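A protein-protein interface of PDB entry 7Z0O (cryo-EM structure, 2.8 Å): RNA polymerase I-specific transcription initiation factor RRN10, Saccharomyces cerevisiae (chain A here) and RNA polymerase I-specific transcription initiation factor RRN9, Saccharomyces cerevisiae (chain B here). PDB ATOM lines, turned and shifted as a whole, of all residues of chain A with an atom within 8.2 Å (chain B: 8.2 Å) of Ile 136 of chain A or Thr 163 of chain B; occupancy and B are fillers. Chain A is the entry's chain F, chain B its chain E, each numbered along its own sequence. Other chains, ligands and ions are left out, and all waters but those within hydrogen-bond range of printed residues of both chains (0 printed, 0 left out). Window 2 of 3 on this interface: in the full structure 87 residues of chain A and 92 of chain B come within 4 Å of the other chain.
N of Asp 165 of chain B is in hydrogen-bond range of O of Ile 132 of chain A (3.1 Å).
The backbone carbonyl oxygen (O) of Thr 163 of chain B is in hydrogen-bond range of the backbone NH (N) of Lys 134 of chain A.
O of Ala 157 of chain B is in hydrogen-bond range of N of Val 162 of chain B, at 2.9 Å.
The side-chain hydroxyl of Ser 133 of chain A sits at hydrogen-bond distance from the backbone carbonyl oxygen of Glu 130 of chain A, at 2.9 Å.
Among the printed residues, merely in contact across the chains: Glu 130 of chain A with Val 162 of chain B (3.3 Å), Ser 133 of chain A with Thr 163 of chain B (3.5 Å), Lys 134 of chain A with Asp 165 of chain B (3.6 Å), Ile 132 of chain A with Leu 164 of chain B (3.7 Å), Ile 132 of chain A with Leu 169 of chain B (3.8 Å), Cys 129 of chain A with Val 162 of chain B (3.8 Å), Cys 129 of chain A with Leu 164 of chain B (3.8 Å), Ile 136 of chain A with Thr 163 of chain B (3.9 Å) and Ser 133 of chain A with Val 162 of chain B (3.9 Å).
Ile 136 of chain A touches one residue of chain B.
Of the printed residues of chain A, Leu 169 of chain B touches Ile 132.
Printed residues of chain A within 4 Å of Asp 165 of chain B: Ile 132 (3.1 Å) and Lys 134 (3.6 Å).
Of the printed residues of chain A, Leu 164 of chain B touches Cys 129 (3.8 Å) and Ile 132 (3.7 Å).
Arg 139 of chain A touches none of the printed residues of chain B.
The nearest residue of chain A that does not touch Thr 163 of chain B is Ile 132 of chain A (4.6 Å).
The nearest printed residue of chain A that does not touch Leu 169 of chain B is Cys 129 of chain A (7.7 Å).
Hydrophobic or aromatic side chains of chain A within 4 Å of the printed part of chain B: Ile 132 and Ile 136.
Of the 10 printed residues of chain B, 5 touch a printed residue of chain A.
Hydrophobic or aromatic side chains of chain B within 4 Å of the printed part of chain A: Val 162, Leu 164 and Leu 169.
Among the printed residues, 11 pairs touch across the chains.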
ATOM      1  N   CYS A 129     -21.341  20.005  12.053  1.00  0.00           N
ATOM      2  CA  CYS A 129     -22.100  20.171  13.288  1.00  0.00           C
ATOM      3  C   CYS A 129     -21.245  20.804  14.379  1.00  0.00           C
ATOM      4  O   CYS A 129     -21.665  21.766  15.032  1.00  0.00           O
ATOM      5  CB  CYS A 129     -22.651  18.820  13.745  1.00  0.00           C
ATOM      6  SG  CYS A 129     -23.169  17.738  12.395  1.00  0.00           S
ATOM      7  N   GLU A 130     -20.035  20.279  14.590  1.00  0.00           N
ATOM      8  CA  GLU A 130     -19.167  20.815  15.635  1.00  0.00           C
ATOM      9  C   GLU A 130     -18.639  22.198  15.288  1.00  0.00           C
ATOM     10  O   GLU A 130     -18.336  22.984  16.191  1.00  0.00           O
ATOM     11  CB  GLU A 130     -18.005  19.859  15.902  1.00  0.00           C
ATOM     12  CG  GLU A 130     -18.286  18.765  16.931  1.00  0.00           C
ATOM     13  CD  GLU A 130     -19.286  17.713  16.481  1.00  0.00           C
ATOM     14  OE1 GLU A 130     -19.241  16.598  17.041  1.00  0.00           O
ATOM     15  OE2 GLU A 130     -20.110  17.975  15.583  1.00  0.00           O
ATOM     16  N   PHE A 131     -18.521  22.515  13.999  1.00  0.00           N
ATOM     17  CA  PHE A 131     -17.996  23.817  13.607  1.00  0.00           C
ATOM     18  C   PHE A 131     -18.894  24.951  14.083  1.00  0.00           C
ATOM     19  O   PHE A 131     -18.429  26.083  14.253  1.00  0.00           O
ATOM     20  CB  PHE A 131     -17.821  23.874  12.092  1.00  0.00           C
ATOM     21  CG  PHE A 131     -17.251  25.165  11.600  1.00  0.00           C
ATOM     22  CD1 PHE A 131     -15.923  25.476  11.819  1.00  0.00           C
ATOM     23  CD2 PHE A 131     -18.044  26.071  10.922  1.00  0.00           C
ATOM     24  CE1 PHE A 131     -15.395  26.667  11.369  1.00  0.00           C
ATOM     25  CE2 PHE A 131     -17.522  27.264  10.471  1.00  0.00           C
ATOM     26  CZ  PHE A 131     -16.196  27.562  10.695  1.00  0.00           C
ATOM     27  N   ILE A 132     -20.175  24.673  14.306  1.00  0.00           N
ATOM     28  CA  ILE A 132     -21.112  25.680  14.786  1.00  0.00           C
ATOM     29  C   ILE A 132     -21.753  25.188  16.076  1.00  0.00           C
ATOM     30  O   ILE A 132     -22.874  25.582  16.416  1.00  0.00           O
ATOM     31  CB  ILE A 132     -22.176  26.000  13.724  1.00  0.00           C
ATOM     32  CG1 ILE A 132     -22.912  24.727  13.311  1.00  0.00           C
ATOM     33  CG2 ILE A 132     -21.538  26.649  12.513  1.00  0.00           C
ATOM     34  CD1 ILE A 132     -24.122  24.981  12.451  1.00  0.00           C
ATOM     35  N   SER A 133     -21.042  24.333  16.804  1.00  0.00           N
ATOM     36  CA  SER A 133     -21.587  23.718  18.003  1.00  0.00           C
ATOM     37  C   SER A 133     -21.681  24.730  19.141  1.00  0.00           C
ATOM     38  O   SER A 133     -21.039  25.783  19.138  1.00  0.00           O
ATOM     39  CB  SER A 133     -20.728  22.532  18.435  1.00  0.00           C
ATOM     40  OG  SER A 133     -19.446  22.966  18.855  1.00  0.00           O
ATOM     41  N   LYS A 134     -22.508  24.391  20.128  1.00  0.00           N
ATOM     42  CA  LYS A 134     -22.653  25.204  21.334  1.00  0.00           C
ATOM     43  C   LYS A 134     -23.269  24.337  22.419  1.00  0.00           C
ATOM     44  O   LYS A 134     -24.424  23.919  22.290  1.00  0.00           O
ATOM     45  CB  LYS A 134     -23.521  26.432  21.064  1.00  0.00           C
ATOM     46  CG  LYS A 134     -23.998  27.151  22.312  1.00  0.00           C
ATOM     47  CD  LYS A 134     -24.446  28.566  21.992  1.00  0.00           C
ATOM     48  CE  LYS A 134     -24.694  29.368  23.256  1.00  0.00           C
ATOM     49  NZ  LYS A 134     -24.292  30.790  23.096  1.00  0.00           N
ATOM     50  N   HIS A 135     -22.512  24.069  23.479  1.00  0.00           N
ATOM     51  CA  HIS A 135     -23.028  23.310  24.610  1.00  0.00           C
ATOM     52  C   HIS A 135     -23.775  24.245  25.550  1.00  0.00           C
ATOM     53  O   HIS A 135     -23.223  25.251  26.006  1.00  0.00           O
ATOM     54  CB  HIS A 135     -21.906  22.578  25.349  1.00  0.00           C
ATOM     55  CG  HIS A 135     -20.822  22.054  24.458  1.00  0.00           C
ATOM     56  ND1 HIS A 135     -20.058  22.864  23.644  1.00  0.00           N
ATOM     57  CD2 HIS A 135     -20.378  20.792  24.251  1.00  0.00           C
ATOM     58  CE1 HIS A 135     -19.196  22.122  22.972  1.00  0.00           C
ATOM     59  NE2 HIS A 135     -19.366  20.862  23.326  1.00  0.00           N
ATOM     60  N   ILE A 136     -25.030  23.910  25.836  1.00  0.00           N
ATOM     61  CA  ILE A 136     -25.911  24.737  26.649  1.00  0.00           C
ATOM     62  C   ILE A 136     -26.359  23.928  27.855  1.00  0.00           C
ATOM     63  O   ILE A 136     -26.745  22.761  27.717  1.00  0.00           O
ATOM     64  CB  ILE A 136     -27.133  25.229  25.850  1.00  0.00           C
ATOM     65  CG1 ILE A 136     -26.773  25.404  24.373  1.00  0.00           C
ATOM     66  CG2 ILE A 136     -27.661  26.527  26.432  1.00  0.00           C
ATOM     67  CD1 ILE A 136     -27.907  25.935  23.528  1.00  0.00           C
ATOM     68  N   ASP A 137     -26.306  24.544  29.034  1.00  0.00           N
ATOM     69  CA  ASP A 137     -26.790  23.943  30.278  1.00  0.00           C
ATOM     70  C   ASP A 137     -27.922  24.831  30.786  1.00  0.00           C
ATOM     71  O   ASP A 137     -27.695  25.750  31.576  1.00  0.00           O
ATOM     72  CB  ASP A 137     -25.669  23.802  31.301  1.00  0.00           C
ATOM     73  CG  ASP A 137     -25.960  22.736  32.339  1.00  0.00           C
ATOM     74  OD1 ASP A 137     -27.104  22.682  32.837  1.00  0.00           O
ATOM     75  OD2 ASP A 137     -25.043  21.949  32.657  1.00  0.00           O
ATOM     76  N   TYR A 138     -29.143  24.551  30.326  1.00  0.00           N
ATOM     77  CA  TYR A 138     -30.290  25.374  30.691  1.00  0.00           C
ATOM     78  C   TYR A 138     -30.648  25.259  32.167  1.00  0.00           C
ATOM     79  O   TYR A 138     -31.345  26.135  32.690  1.00  0.00           O
ATOM     80  CB  TYR A 138     -31.497  24.999  29.831  1.00  0.00           C
ATOM     81  CG  TYR A 138     -31.386  25.466  28.397  1.00  0.00           C
ATOM     82  CD1 TYR A 138     -31.307  26.818  28.092  1.00  0.00           C
ATOM     83  CD2 TYR A 138     -31.355  24.555  27.350  1.00  0.00           C
ATOM     84  CE1 TYR A 138     -31.204  27.250  26.785  1.00  0.00           C
ATOM     85  CE2 TYR A 138     -31.252  24.978  26.039  1.00  0.00           C
ATOM     86  CZ  TYR A 138     -31.177  26.327  25.762  1.00  0.00           C
ATOM     87  OH  TYR A 138     -31.074  26.755  24.460  1.00  0.00           O
ATOM     88  N   ARG A 139     -30.195  24.201  32.845  1.00  0.00           N
ATOM     89  CA  ARG A 139     -30.492  24.052  34.265  1.00  0.00           C
ATOM     90  C   ARG A 139     -29.848  25.163  35.083  1.00  0.00           C
ATOM     91  O   ARG A 139     -30.464  25.699  36.012  1.00  0.00           O
ATOM     92  CB  ARG A 139     -30.021  22.684  34.759  1.00  0.00           C
ATOM     93  CG  ARG A 139     -30.883  21.523  34.297  1.00  0.00           C
ATOM     94  CD  ARG A 139     -30.288  20.861  33.065  1.00  0.00           C
ATOM     95  NE  ARG A 139     -31.096  19.742  32.596  1.00  0.00           N
ATOM     96  CZ  ARG A 139     -31.990  19.821  31.621  1.00  0.00           C
ATOM     97  NH1 ARG A 139     -32.219  20.958  30.984  1.00  0.00           N
ATOM     98  NH2 ARG A 139     -32.672  18.733  31.276  1.00  0.00           N
ATOM     99  N   HIS A 140     -28.609  25.524  34.753  1.00  0.00           N
ATOM    100  CA  HIS A 140     -27.871  26.543  35.487  1.00  0.00           C
ATOM    101  C   HIS A 140     -27.635  27.819  34.699  1.00  0.00           C
ATOM    102  O   HIS A 140     -27.524  28.888  35.303  1.00  0.00           O
ATOM    103  CB  HIS A 140     -26.516  25.987  35.945  1.00  0.00           C
ATOM    104  CG  HIS A 140     -26.568  24.556  36.381  1.00  0.00           C
ATOM    105  ND1 HIS A 140     -26.450  23.505  35.497  1.00  0.00           N
ATOM    106  CD2 HIS A 140     -26.726  24.002  37.605  1.00  0.00           C
ATOM    107  CE1 HIS A 140     -26.534  22.364  36.159  1.00  0.00           C
ATOM    108  NE2 HIS A 140     -26.702  22.638  37.440  1.00  0.00           N
ATOM    109  N   ALA A 141     -27.555  27.740  33.373  1.00  0.00           N
ATOM    110  CA  ALA A 141     -27.315  28.903  32.518  1.00  0.00           C
ATOM    111  C   ALA A 141     -28.360  28.941  31.410  1.00  0.00           C
ATOM    112  O   ALA A 141     -28.070  28.626  30.249  1.00  0.00           O
ATOM    113  CB  ALA A 141     -25.901  28.873  31.938  1.00  0.00           C
ATOM    114  N   PRO A 142     -29.597  29.327  31.737  1.00  0.00           N
ATOM    115  CA  PRO A 142     -30.641  29.398  30.703  1.00  0.00           C
ATOM    116  C   PRO A 142     -30.515  30.601  29.784  1.00  0.00           C
ATOM    117  O   PRO A 142     -31.239  30.668  28.784  1.00  0.00           O
ATOM    118  CB  PRO A 142     -31.934  29.461  31.521  1.00  0.00           C
ATOM    119  CG  PRO A 142     -31.527  30.134  32.787  1.00  0.00           C
ATOM    120  CD  PRO A 142     -30.104  29.720  33.063  1.00  0.00           C
ATOM    121  N   GLY A 143     -29.627  31.548  30.086  1.00  0.00           N
ATOM    122  CA  GLY A 143     -29.493  32.742  29.273  1.00  0.00           C
ATOM    123  C   GLY A 143     -28.695  32.578  27.997  1.00  0.00           C
ATOM    124  O   GLY A 143     -28.680  33.500  27.176  1.00  0.00           O
ATOM    125  N   ASN A 144     -28.026  31.438  27.813  1.00  0.00           N
ATOM    126  CA  ASN A 144     -27.266  31.221  26.585  1.00  0.00           C
ATOM    127  C   ASN A 144     -28.187  31.160  25.373  1.00  0.00           C
ATOM    128  O   ASN A 144     -27.982  31.879  24.387  1.00  0.00           O
ATOM    129  CB  ASN A 144     -26.441  29.939  26.696  1.00  0.00           C
ATOM    130  CG  ASN A 144     -25.323  30.051  27.710  1.00  0.00           C
ATOM    131  OD1 ASN A 144     -25.297  29.329  28.704  1.00  0.00           O
ATOM    132  ND2 ASN A 144     -24.389  30.961  27.461  1.00  0.00           N
ATOM    133  N   ILE A 145     -29.214  30.315  25.437  1.00  0.00           N
ATOM    134  CA  ILE A 145     -30.176  30.137  24.351  1.00  0.00           C
ATOM    135  C   ILE A 145     -29.478  29.834  23.029  1.00  0.00           C
ATOM    136  O   ILE A 145     -29.825  28.877  22.336  1.00  0.00           O
ATOM    137  CB  ILE A 145     -31.089  31.370  24.213  1.00  0.00           C
ATOM    138  CG1 ILE A 145     -31.961  31.526  25.459  1.00  0.00           C
ATOM    139  CG2 ILE A 145     -31.951  31.258  22.968  1.00  0.00           C
ATOM    140  CD1 ILE A 145     -32.809  32.776  25.458  1.00  0.00           C
ATOM    141  N   ALA B 157     -27.001  16.861  13.168  1.00  0.00           N
ATOM    142  CA  ALA B 157     -26.637  17.112  14.559  1.00  0.00           C
ATOM    143  C   ALA B 157     -27.317  16.123  15.496  1.00  0.00           C
ATOM    144  O   ALA B 157     -26.703  15.635  16.451  1.00  0.00           O
ATOM    145  CB  ALA B 157     -26.993  18.548  14.943  1.00  0.00           C
ATOM    146  N   LEU B 158     -28.592  15.821  15.244  1.00  0.00           N
ATOM    147  CA  LEU B 158     -29.310  14.877  16.095  1.00  0.00           C
ATOM    148  C   LEU B 158     -28.688  13.488  16.029  1.00  0.00           C
ATOM    149  O   LEU B 158     -28.579  12.800  17.050  1.00  0.00           O
ATOM    150  CB  LEU B 158     -30.786  14.823  15.701  1.00  0.00           C
ATOM    151  CG  LEU B 158     -31.759  15.843  16.303  1.00  0.00           C
ATOM    152  CD1 LEU B 158     -31.191  17.254  16.334  1.00  0.00           C
ATOM    153  CD2 LEU B 158     -33.074  15.817  15.544  1.00  0.00           C
ATOM    154  N   HIS B 160     -25.554  12.746  15.379  1.00  0.00           N
ATOM    155  CA  HIS B 160     -24.250  12.798  16.023  1.00  0.00           C
ATOM    156  C   HIS B 160     -24.300  13.411  17.415  1.00  0.00           C
ATOM    157  O   HIS B 160     -23.248  13.590  18.035  1.00  0.00           O
ATOM    158  CB  HIS B 160     -23.267  13.572  15.142  1.00  0.00           C
ATOM    159  CG  HIS B 160     -23.039  12.944  13.802  1.00  0.00           C
ATOM    160  ND1 HIS B 160     -21.803  12.496  13.389  1.00  0.00           N
ATOM    161  CD2 HIS B 160     -23.891  12.686  12.782  1.00  0.00           C
ATOM    162  CE1 HIS B 160     -21.903  11.990  12.173  1.00  0.00           C
ATOM    163  NE2 HIS B 160     -23.161  12.094  11.781  1.00  0.00           N
ATOM    164  N   ASP B 161     -25.495  13.740  17.914  1.00  0.00           N
ATOM    165  CA  ASP B 161     -25.707  14.216  19.281  1.00  0.00           C
ATOM    166  C   ASP B 161     -24.894  15.485  19.557  1.00  0.00           C
ATOM    167  O   ASP B 161     -24.011  15.530  20.415  1.00  0.00           O
ATOM    168  CB  ASP B 161     -25.374  13.116  20.296  1.00  0.00           C
ATOM    169  CG  ASP B 161     -26.262  13.167  21.519  1.00  0.00           C
ATOM    170  OD1 ASP B 161     -27.495  13.271  21.352  1.00  0.00           O
ATOM    171  OD2 ASP B 161     -25.729  13.104  22.646  1.00  0.00           O
ATOM    172  N   VAL B 162     -25.225  16.526  18.798  1.00  0.00           N
ATOM    173  CA  VAL B 162     -24.558  17.819  18.906  1.00  0.00           C
ATOM    174  C   VAL B 162     -25.618  18.905  19.012  1.00  0.00           C
ATOM    175  O   VAL B 162     -26.581  18.918  18.239  1.00  0.00           O
ATOM    176  CB  VAL B 162     -23.630  18.085  17.704  1.00  0.00           C
ATOM    177  CG1 VAL B 162     -23.128  19.519  17.723  1.00  0.00           C
ATOM    178  CG2 VAL B 162     -22.470  17.109  17.706  1.00  0.00           C
ATOM    179  N   THR B 163     -25.448  19.809  19.972  1.00  0.00           N
ATOM    180  CA  THR B 163     -26.313  20.974  20.077  1.00  0.00           C
ATOM    181  C   THR B 163     -25.762  22.101  19.216  1.00  0.00           C
ATOM    182  O   THR B 163     -24.560  22.380  19.230  1.00  0.00           O
ATOM    183  CB  THR B 163     -26.426  21.428  21.532  1.00  0.00           C
ATOM    184  OG1 THR B 163     -26.898  20.341  22.337  1.00  0.00           O
ATOM    185  CG2 THR B 163     -27.392  22.594  21.653  1.00  0.00           C
ATOM    186  N   LEU B 164     -26.644  22.745  18.461  1.00  0.00           N
ATOM    187  CA  LEU B 164     -26.243  23.766  17.506  1.00  0.00           C
ATOM    188  C   LEU B 164     -26.490  25.163  18.060  1.00  0.00           C
ATOM    189  O   LEU B 164     -27.466  25.408  18.773  1.00  0.00           O
ATOM    190  CB  LEU B 164     -26.994  23.605  16.183  1.00  0.00           C
ATOM    191  CG  LEU B 164     -26.775  22.307  15.409  1.00  0.00           C
ATOM    192  CD1 LEU B 164     -27.914  22.083  14.434  1.00  0.00           C
ATOM    193  CD2 LEU B 164     -25.441  22.333  14.683  1.00  0.00           C
ATOM    194  N   ASP B 165     -25.589  26.078  17.721  1.00  0.00           N
ATOM    195  CA  ASP B 165     -25.780  27.486  18.030  1.00  0.00           C
ATOM    196  C   ASP B 165     -26.711  28.098  16.995  1.00  0.00           C
ATOM    197  O   ASP B 165     -26.431  28.058  15.793  1.00  0.00           O
ATOM    198  CB  ASP B 165     -24.440  28.220  18.048  1.00  0.00           C
ATOM    199  CG  ASP B 165     -24.580  29.687  18.406  1.00  0.00           C
ATOM    200  OD1 ASP B 165     -25.625  30.069  18.973  1.00  0.00           O
ATOM    201  OD2 ASP B 165     -23.641  30.460  18.124  1.00  0.00           O
ATOM    202  N   VAL B 166     -27.822  28.667  17.464  1.00  0.00           N
ATOM    203  CA  VAL B 166     -28.849  29.163  16.552  1.00  0.00           C
ATOM    204  C   VAL B 166     -28.459  30.456  15.859  1.00  0.00           C
ATOM    205  O   VAL B 166     -29.156  30.882  14.931  1.00  0.00           O
ATOM    206  CB  VAL B 166     -30.175  29.354  17.309  1.00  0.00           C
ATOM    207  CG1 VAL B 166     -30.749  28.003  17.704  1.00  0.00           C
ATOM    208  CG2 VAL B 166     -29.959  30.219  18.535  1.00  0.00           C
ATOM    209  N   LEU B 169     -26.632  29.258  12.151  1.00  0.00           N
ATOM    210  CA  LEU B 169     -27.248  28.296  11.245  1.00  0.00           C
ATOM    211  C   LEU B 169     -27.502  28.863   9.856  1.00  0.00           C
ATOM    212  O   LEU B 169     -27.843  28.095   8.951  1.00  0.00           O
ATOM    213  CB  LEU B 169     -28.561  27.788  11.837  1.00  0.00           C
ATOM    214  CG  LEU B 169     -28.435  26.720  12.922  1.00  0.00           C
ATOM    215  CD1 LEU B 169     -29.777  26.474  13.584  1.00  0.00           C
ATOM    216  CD2 LEU B 169     -27.883  25.437  12.332  1.00  0.00           C
